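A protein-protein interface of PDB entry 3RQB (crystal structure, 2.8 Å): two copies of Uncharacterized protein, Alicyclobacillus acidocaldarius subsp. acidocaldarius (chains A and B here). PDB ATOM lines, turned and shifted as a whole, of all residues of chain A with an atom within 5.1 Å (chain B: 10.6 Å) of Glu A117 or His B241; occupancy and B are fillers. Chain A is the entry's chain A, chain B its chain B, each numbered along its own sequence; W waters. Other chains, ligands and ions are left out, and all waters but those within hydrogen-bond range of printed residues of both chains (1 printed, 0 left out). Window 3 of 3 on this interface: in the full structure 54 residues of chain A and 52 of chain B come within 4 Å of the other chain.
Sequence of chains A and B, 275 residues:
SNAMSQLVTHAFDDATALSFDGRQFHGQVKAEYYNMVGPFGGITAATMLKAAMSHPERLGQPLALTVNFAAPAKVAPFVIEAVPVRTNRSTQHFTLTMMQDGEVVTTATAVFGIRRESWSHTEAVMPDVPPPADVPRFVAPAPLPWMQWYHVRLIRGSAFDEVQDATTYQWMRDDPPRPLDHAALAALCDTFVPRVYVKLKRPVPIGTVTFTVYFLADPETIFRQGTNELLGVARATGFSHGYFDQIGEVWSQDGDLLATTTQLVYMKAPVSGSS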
ATOM      1  N   ARG A 115      34.248   8.753  15.207  1.00  0.00           N
ATOM      2  CA  ARG A 115      32.793   8.828  15.203  1.00  0.00           C
ATOM      3  C   ARG A 115      32.346  10.026  16.025  1.00  0.00           C
ATOM      4  O   ARG A 115      32.689  10.133  17.209  1.00  0.00           O
ATOM      5  CB  ARG A 115      32.189   7.557  15.812  1.00  0.00           C
ATOM      6  CG  ARG A 115      32.659   6.261  15.173  1.00  0.00           C
ATOM      7  CD  ARG A 115      32.285   6.207  13.698  1.00  0.00           C
ATOM      8  NE  ARG A 115      30.841   6.134  13.489  1.00  0.00           N
ATOM      9  CZ  ARG A 115      30.160   4.997  13.391  1.00  0.00           C
ATOM     10  NH1 ARG A 115      30.785   3.829  13.483  1.00  0.00           N
ATOM     11  NH2 ARG A 115      28.850   5.024  13.200  1.00  0.00           N
ATOM     12  N   ARG A 116      31.578  10.917  15.401  1.00  0.00           N
ATOM     13  CA  ARG A 116      31.060  12.105  16.082  1.00  0.00           C
ATOM     14  C   ARG A 116      29.548  12.046  16.288  1.00  0.00           C
ATOM     15  O   ARG A 116      28.820  11.440  15.496  1.00  0.00           O
ATOM     16  CB  ARG A 116      31.441  13.366  15.315  1.00  0.00           C
ATOM     17  CG  ARG A 116      32.937  13.587  15.244  1.00  0.00           C
ATOM     18  CD  ARG A 116      33.268  14.926  14.600  1.00  0.00           C
ATOM     19  NE  ARG A 116      34.245  15.671  15.392  1.00  0.00           N
ATOM     20  CZ  ARG A 116      35.552  15.695  15.146  1.00  0.00           C
ATOM     21  NH1 ARG A 116      36.062  15.025  14.119  1.00  0.00           N
ATOM     22  NH2 ARG A 116      36.351  16.401  15.928  1.00  0.00           N
ATOM     23  N   GLU A 117      29.071  12.666  17.360  1.00  0.00           N
ATOM     24  CA  GLU A 117      27.644  12.631  17.619  1.00  0.00           C
ATOM     25  C   GLU A 117      26.926  13.272  16.441  1.00  0.00           C
ATOM     26  O   GLU A 117      27.328  14.328  15.958  1.00  0.00           O
ATOM     27  CB  GLU A 117      27.287  13.307  18.945  1.00  0.00           C
ATOM     28  CG  GLU A 117      25.998  12.763  19.568  1.00  0.00           C
ATOM     29  CD  GLU A 117      25.906  11.233  19.513  1.00  0.00           C
ATOM     30  OE1 GLU A 117      26.399  10.560  20.450  1.00  0.00           O
ATOM     31  OE2 GLU A 117      25.332  10.702  18.531  1.00  0.00           O
ATOM     32  N   SER A 118      25.878  12.609  15.966  1.00  0.00           N
ATOM     33  CA  SER A 118      25.200  13.029  14.750  1.00  0.00           C
ATOM     34  C   SER A 118      23.834  12.385  14.677  1.00  0.00           C
ATOM     35  O   SER A 118      23.463  11.611  15.558  1.00  0.00           O
ATOM     36  CB  SER A 118      26.015  12.616  13.519  1.00  0.00           C
ATOM     37  OG  SER A 118      25.782  11.254  13.173  1.00  0.00           O
ATOM     38  N   TRP A 119      23.097  12.695  13.614  1.00  0.00           N
ATOM     39  CA  TRP A 119      21.770  12.128  13.395  1.00  0.00           C
ATOM     40  C   TRP A 119      21.803  10.607  13.305  1.00  0.00           C
ATOM     41  O   TRP A 119      22.743  10.032  12.750  1.00  0.00           O
ATOM     42  CB  TRP A 119      21.120  12.705  12.131  1.00  0.00           C
ATOM     43  CG  TRP A 119      19.775  12.089  11.837  1.00  0.00           C
ATOM     44  CD1 TRP A 119      18.648  12.152  12.618  1.00  0.00           C
ATOM     45  CD2 TRP A 119      19.421  11.308  10.692  1.00  0.00           C
ATOM     46  NE1 TRP A 119      17.620  11.453  12.027  1.00  0.00           N
ATOM     47  CE2 TRP A 119      18.069  10.927  10.840  1.00  0.00           C
ATOM     48  CE3 TRP A 119      20.117  10.883   9.557  1.00  0.00           C
ATOM     49  CZ2 TRP A 119      17.402  10.149   9.895  1.00  0.00           C
ATOM     50  CZ3 TRP A 119      19.450  10.108   8.614  1.00  0.00           C
ATOM     51  CH2 TRP A 119      18.111   9.750   8.789  1.00  0.00           C
ATOM     52  N   SER A 120      20.777   9.962  13.859  1.00  0.00           N
ATOM     53  CA  SER A 120      20.672   8.507  13.800  1.00  0.00           C
ATOM     54  C   SER A 120      19.286   8.010  13.404  1.00  0.00           C
ATOM     55  O   SER A 120      18.268   8.451  13.944  1.00  0.00           O
ATOM     56  CB  SER A 120      21.108   7.867  15.125  1.00  0.00           C
ATOM     57  OG  SER A 120      22.522   7.901  15.264  1.00  0.00           O
ATOM     58  N   ASP A 218      28.970   3.143  17.014  1.00  0.00           N
ATOM     59  CA  ASP A 218      30.118   3.887  17.480  1.00  0.00           C
ATOM     60  C   ASP A 218      30.804   3.044  18.555  1.00  0.00           C
ATOM     61  O   ASP A 218      30.192   2.146  19.140  1.00  0.00           O
ATOM     62  CB  ASP A 218      29.703   5.268  17.991  1.00  0.00           C
ATOM     63  CG  ASP A 218      29.384   5.274  19.459  1.00  0.00           C
ATOM     64  OD1 ASP A 218      28.276   4.835  19.826  1.00  0.00           O
ATOM     65  OD2 ASP A 218      30.248   5.734  20.242  1.00  0.00           O
ATOM     66  N   GLU A 220      31.677   3.583  21.643  1.00  0.00           N
ATOM     67  CA  GLU A 220      31.003   3.532  22.942  1.00  0.00           C
ATOM     68  C   GLU A 220      29.896   2.466  22.964  1.00  0.00           C
ATOM     69  O   GLU A 220      29.700   1.801  23.974  1.00  0.00           O
ATOM     70  CB  GLU A 220      30.499   4.913  23.393  1.00  0.00           C
ATOM     71  CG  GLU A 220      29.060   5.280  23.037  1.00  0.00           C
ATOM     72  CD  GLU A 220      28.681   6.683  23.539  1.00  0.00           C
ATOM     73  OE1 GLU A 220      27.500   7.083  23.403  1.00  0.00           O
ATOM     74  OE2 GLU A 220      29.572   7.387  24.072  1.00  0.00           O
ATOM     75  N   VAL B 209      34.052   6.324   1.984  1.00  0.00           N
ATOM     76  CA  VAL B 209      35.324   5.825   2.472  1.00  0.00           C
ATOM     77  C   VAL B 209      35.745   4.543   1.757  1.00  0.00           C
ATOM     78  O   VAL B 209      36.913   4.373   1.390  1.00  0.00           O
ATOM     79  CB  VAL B 209      35.225   5.540   3.965  1.00  0.00           C
ATOM     80  CG1 VAL B 209      36.469   4.795   4.458  1.00  0.00           C
ATOM     81  CG2 VAL B 209      35.002   6.840   4.709  1.00  0.00           C
ATOM     82  N   GLY B 238      21.689   1.295   8.340  1.00  0.00           N
ATOM     83  CA  GLY B 238      21.528   2.245   9.418  1.00  0.00           C
ATOM     84  C   GLY B 238      22.334   3.499   9.179  1.00  0.00           C
ATOM     85  O   GLY B 238      23.132   3.563   8.245  1.00  0.00           O
ATOM     86  N   PHE B 239      22.092   4.508  10.011  1.00  0.00           N
ATOM     87  CA  PHE B 239      22.860   5.736   9.988  1.00  0.00           C
ATOM     88  C   PHE B 239      23.215   6.057  11.428  1.00  0.00           C
ATOM     89  O   PHE B 239      22.325   6.313  12.243  1.00  0.00           O
ATOM     90  CB  PHE B 239      22.014   6.877   9.436  1.00  0.00           C
ATOM     91  CG  PHE B 239      21.304   6.562   8.136  1.00  0.00           C
ATOM     92  CD1 PHE B 239      20.084   5.891   8.134  1.00  0.00           C
ATOM     93  CD2 PHE B 239      21.829   6.981   6.917  1.00  0.00           C
ATOM     94  CE1 PHE B 239      19.413   5.620   6.933  1.00  0.00           C
ATOM     95  CE2 PHE B 239      21.164   6.714   5.713  1.00  0.00           C
ATOM     96  CZ  PHE B 239      19.957   6.035   5.723  1.00  0.00           C
ATOM     97  N   SER B 240      24.497   6.058  11.762  1.00  0.00           N
ATOM     98  CA  SER B 240      24.853   6.362  13.138  1.00  0.00           C
ATOM     99  C   SER B 240      26.154   7.123  13.266  1.00  0.00           C
ATOM    100  O   SER B 240      27.109   6.852  12.543  1.00  0.00           O
ATOM    101  CB  SER B 240      24.921   5.084  13.970  1.00  0.00           C
ATOM    102  OG  SER B 240      25.293   5.375  15.306  1.00  0.00           O
ATOM    103  N   HIS B 241      26.167   8.095  14.170  1.00  0.00           N
ATOM    104  CA  HIS B 241      27.406   8.719  14.606  1.00  0.00           C
ATOM    105  C   HIS B 241      28.346   9.043  13.453  1.00  0.00           C
ATOM    106  O   HIS B 241      29.538   8.731  13.509  1.00  0.00           O
ATOM    107  CB  HIS B 241      28.113   7.837  15.632  1.00  0.00           C
ATOM    108  CG  HIS B 241      27.479   7.863  16.985  1.00  0.00           C
ATOM    109  ND1 HIS B 241      26.186   7.442  17.208  1.00  0.00           N
ATOM    110  CD2 HIS B 241      27.958   8.261  18.189  1.00  0.00           C
ATOM    111  CE1 HIS B 241      25.897   7.577  18.489  1.00  0.00           C
ATOM    112  NE2 HIS B 241      26.955   8.073  19.107  1.00  0.00           N
ATOM    113  N   GLY B 242      27.814   9.643  12.395  1.00  0.00           N
ATOM    114  CA  GLY B 242      28.664  10.148  11.337  1.00  0.00           C
ATOM    115  C   GLY B 242      28.828   9.265  10.121  1.00  0.00           C
ATOM    116  O   GLY B 242      29.464   9.672   9.153  1.00  0.00           O
ATOM    117  N   TYR B 243      28.269   8.061  10.148  1.00  0.00           N
ATOM    118  CA  TYR B 243      28.373   7.183   8.982  1.00  0.00           C
ATOM    119  C   TYR B 243      27.094   6.449   8.626  1.00  0.00           C
ATOM    120  O   TYR B 243      26.184   6.315   9.448  1.00  0.00           O
ATOM    121  CB  TYR B 243      29.504   6.170   9.154  1.00  0.00           C
ATOM    122  CG  TYR B 243      30.860   6.814   9.095  1.00  0.00           C
ATOM    123  CD1 TYR B 243      31.579   6.876   7.908  1.00  0.00           C
ATOM    124  CD2 TYR B 243      31.409   7.392  10.227  1.00  0.00           C
ATOM    125  CE1 TYR B 243      32.829   7.484   7.865  1.00  0.00           C
ATOM    126  CE2 TYR B 243      32.640   7.999  10.198  1.00  0.00           C
ATOM    127  CZ  TYR B 243      33.357   8.045   9.023  1.00  0.00           C
ATOM    128  OH  TYR B 243      34.600   8.661   9.044  1.00  0.00           O
ATOM    129  N   PHE B 244      27.032   5.990   7.380  1.00  0.00           N
ATOM    130  CA  PHE B 244      25.984   5.072   6.960  1.00  0.00           C
ATOM    131  C   PHE B 244      26.494   4.181   5.832  1.00  0.00           C
ATOM    132  O   PHE B 244      27.583   4.406   5.299  1.00  0.00           O
ATOM    133  CB  PHE B 244      24.754   5.846   6.484  1.00  0.00           C
ATOM    134  CG  PHE B 244      24.932   6.481   5.138  1.00  0.00           C
ATOM    135  CD1 PHE B 244      25.398   7.784   5.031  1.00  0.00           C
ATOM    136  CD2 PHE B 244      24.645   5.764   3.973  1.00  0.00           C
ATOM    137  CE1 PHE B 244      25.568   8.364   3.786  1.00  0.00           C
ATOM    138  CE2 PHE B 244      24.813   6.329   2.725  1.00  0.00           C
ATOM    139  CZ  PHE B 244      25.275   7.631   2.626  1.00  0.00           C
ATOM    140  N   ASP B 245      25.655   3.233   5.416  1.00  0.00           N
ATOM    141  CA  ASP B 245      26.062   2.185   4.490  1.00  0.00           C
ATOM    142  C   ASP B 245      25.050   1.973   3.368  1.00  0.00           C
ATOM    143  O   ASP B 245      23.870   2.293   3.496  1.00  0.00           O
ATOM    144  CB  ASP B 245      26.247   0.864   5.240  1.00  0.00           C
ATOM    145  CG  ASP B 245      24.945   0.099   5.395  1.00  0.00           C
ATOM    146  OD1 ASP B 245      23.904   0.733   5.673  1.00  0.00           O
ATOM    147  OD2 ASP B 245      24.963  -1.135   5.217  1.00  0.00           O
ATOM    148  N   LEU B 264      30.493   2.052   2.373  1.00  0.00           N
ATOM    149  CA  LEU B 264      30.500   2.734   3.659  1.00  0.00           C
ATOM    150  C   LEU B 264      30.714   4.217   3.411  1.00  0.00           C
ATOM    151  O   LEU B 264      31.678   4.620   2.758  1.00  0.00           O
ATOM    152  CB  LEU B 264      31.589   2.193   4.578  1.00  0.00           C
ATOM    153  CG  LEU B 264      31.511   2.820   5.975  1.00  0.00           C
ATOM    154  CD1 LEU B 264      30.128   2.586   6.557  1.00  0.00           C
ATOM    155  CD2 LEU B 264      32.599   2.306   6.932  1.00  0.00           C
ATOM    156  N   VAL B 265      29.814   5.037   3.929  1.00  0.00           N
ATOM    157  CA  VAL B 265      29.837   6.430   3.563  1.00  0.00           C
ATOM    158  C   VAL B 265      29.792   7.370   4.751  1.00  0.00           C
ATOM    159  O   VAL B 265      28.882   7.318   5.583  1.00  0.00           O
ATOM    160  CB  VAL B 265      28.672   6.752   2.651  1.00  0.00           C
ATOM    161  CG1 VAL B 265      28.863   8.126   2.046  1.00  0.00           C
ATOM    162  CG2 VAL B 265      28.559   5.696   1.577  1.00  0.00           C
ATOM    163  N   TYR B 266      30.794   8.233   4.805  1.00  0.00           N
ATOM    164  CA  TYR B 266      30.818   9.345   5.729  1.00  0.00           C
ATOM    165  C   TYR B 266      29.639  10.277   5.497  1.00  0.00           C
ATOM    166  O   TYR B 266      29.293  10.597   4.363  1.00  0.00           O
ATOM    167  CB  TYR B 266      32.097  10.135   5.539  1.00  0.00           C
ATOM    168  CG  TYR B 266      32.137  11.383   6.376  1.00  0.00           C
ATOM    169  CD1 TYR B 266      32.427  11.320   7.740  1.00  0.00           C
ATOM    170  CD2 TYR B 266      31.883  12.626   5.815  1.00  0.00           C
ATOM    171  CE1 TYR B 266      32.471  12.468   8.526  1.00  0.00           C
ATOM    172  CE2 TYR B 266      31.923  13.780   6.592  1.00  0.00           C
ATOM    173  CZ  TYR B 266      32.219  13.696   7.948  1.00  0.00           C
ATOM    174  OH  TYR B 266      32.260  14.840   8.721  1.00  0.00           O
ATOM    175  N   MET B 267      29.044  10.738   6.583  1.00  0.00           N
ATOM    176  CA  MET B 267      27.873  11.589   6.505  1.00  0.00           C
ATOM    177  C   MET B 267      27.925  12.714   7.551  1.00  0.00           C
ATOM    178  O   MET B 267      28.268  12.472   8.712  1.00  0.00           O
ATOM    179  CB  MET B 267      26.651  10.712   6.695  1.00  0.00           C
ATOM    180  CG  MET B 267      25.465  11.383   7.313  1.00  0.00           C
ATOM    181  SD  MET B 267      24.410   9.990   8.135  1.00  0.00           S
ATOM    182  CE  MET B 267      25.484   9.698   9.749  1.00  0.00           C
ATOM    183  N   LYS B 268      27.591  13.940   7.136  1.00  0.00           N
ATOM    184  CA  LYS B 268      27.711  15.133   7.994  1.00  0.00           C
ATOM    185  C   LYS B 268      26.493  15.640   8.802  1.00  0.00           C
ATOM    186  O   LYS B 268      26.578  16.685   9.431  1.00  0.00           O
ATOM    187  CB  LYS B 268      28.337  16.305   7.226  1.00  0.00           C
ATOM    188  CG  LYS B 268      29.856  16.234   7.140  1.00  0.00           C
ATOM    189  CD  LYS B 268      30.520  17.582   7.380  1.00  0.00           C
ATOM    190  CE  LYS B 268      32.047  17.447   7.543  1.00  0.00           C
ATOM    191  NZ  LYS B 268      32.800  17.214   6.263  1.00  0.00           N
ATOM    192  N   ALA B 269      25.369  14.934   8.788  1.00  0.00           N
ATOM    193  CA  ALA B 269      24.173  15.412   9.499  1.00  0.00           C
ATOM    194  C   ALA B 269      24.285  15.495  11.034  1.00  0.00           C
ATOM    195  O   ALA B 269      24.437  14.478  11.708  1.00  0.00           O
ATOM    196  CB  ALA B 269      22.967  14.564   9.111  1.00  0.00           C
ATOM    197  N   PRO B 270      24.214  16.718  11.586  1.00  0.00           N
ATOM    198  CA  PRO B 270      24.080  16.961  13.024  1.00  0.00           C
ATOM    199  C   PRO B 270      22.619  17.136  13.431  1.00  0.00           C
ATOM    200  O   PRO B 270      21.727  17.082  12.581  1.00  0.00           O
ATOM    201  CB  PRO B 270      24.844  18.266  13.215  1.00  0.00           C
ATOM    202  CG  PRO B 270      24.588  19.010  11.938  1.00  0.00           C
ATOM    203  CD  PRO B 270      24.394  17.978  10.844  1.00  0.00           C
ATOM    204  N   VAL B 271      22.391  17.386  14.718  1.00  0.00           N
ATOM    205  CA  VAL B 271      21.040  17.445  15.278  1.00  0.00           C
ATOM    206  C   VAL B 271      20.469  18.868  15.328  1.00  0.00           C
ATOM    207  O   VAL B 271      19.348  19.091  15.797  1.00  0.00           O
ATOM    208  CB  VAL B 271      21.016  16.841  16.699  1.00  0.00           C
ATOM    209  CG1 VAL B 271      19.583  16.479  17.113  1.00  0.00           C
ATOM    210  CG2 VAL B 271      21.953  15.623  16.776  1.00  0.00           C
HETATM  211  O   HOH W   1      26.234   6.272  21.160  1.00  0.00           O
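Tyr B243 touches Arg A115. Gly B242 touches Arg A116. Met B267 touches Ser A118. CB of Ser A118 touches O of Ala B269 (3.0 Å). O of Trp A119 touches O of Phe B239 (3.8 Å). Ser B240 touches Ser A120 (CA to OG, 3.5 Å). His B241 touches Ser A120. His B241 touches Asp A218 (CD2 to CB, 3.5 Å).
No position is printed for both chains.
OG of Ser B240 is in hydrogen-bond range of ND1 of His B241 (2.9 Å). O of Gly B242 lies within hydrogen-bond range of N of Met B267 (2.8 Å). OD2 of Asp A218 is in hydrogen-bond range of N of Glu A220 (2.9 Å).
O of His B241 lies within hydrogen-bond range of NE of Arg A115 (2.9 Å). OG of Ser A118 sits close to N of His B241, 3.3 Å away. O of Arg A116 sits close to O of His B241, 3.4 Å away. OG of Ser A118 sits at hydrogen-bond distance from N of Gly B242 (2.7 Å). OE1 of Glu A117 lies within hydrogen-bond range of NE2 of His B241 (2.9 Å). The backbone carbonyl oxygen (O) of Ala B269 sits at hydrogen-bond distance from the backbone NH (N) of Trp A119, at 2.9 Å. The guanidinium group of Arg A115 sits at hydrogen-bond distance from the backbone carbonyl oxygen of Ser B240. The side-chain hydroxyl (OG) of Ser A120 sits close to the backbone carbonyl oxygen (O) of Phe B239 (3.4 Å).
Water W1 lies within hydrogen-bond range of the side-chain carboxylate (OE1) of Glu A220, a ring nitrogen (NE2) of His B241 and the side-chain carboxylate (OD1) of Asp A218.
Glu A117 touches one residue of chain B. His B241 touches just these residues of chain A: Arg A115, Arg A116, Glu A117, Ser A118, Ser A120 and Asp A218. Of chain B, only Ser B240 (2.6 Å), His B241 (2.9 Å) and Tyr B243 (3.5 Å) come within 4 Å of Arg A115. Of chain B, only His B241 (3.3 Å), Gly B242 (2.7 Å), Met B267 (3.8 Å) and Ala B269 (3.0 Å) come within 4 Å of Ser A118. Printed residues of chain A within 4 Å of Ala B269: Ser A118 (3.0 Å) and Trp A119 (2.9 Å). Of the printed residues of chain A, Gly B242 touches Arg A116 (3.7 Å) and Ser A118 (2.7 Å). Printed residues of chain B within 4 Å of Ser A120: Phe B239, Ser B240 and His B241. Leu B264 touches none of the printed residues of chain A. The nearest residue of chain B that does not touch Glu A117 is Pro B270 (5.1 Å). The nearest residue of chain A that does not touch His B241 is Trp A119 (4.2 Å).
Of the 17 printed residues of chain B, 7 touch a printed residue of chain A. Hydrophobic or aromatic side chains of chain B that line the printed part of chain A: His B241, Tyr B243, Met B267 and Ala B269. Among the printed residues, 16 pairs touch across the chains. Among the printed residues, no Asp or Glu carboxylate lies within 4 Å of a Lys or Arg side-chain nitrogen of the other chain.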
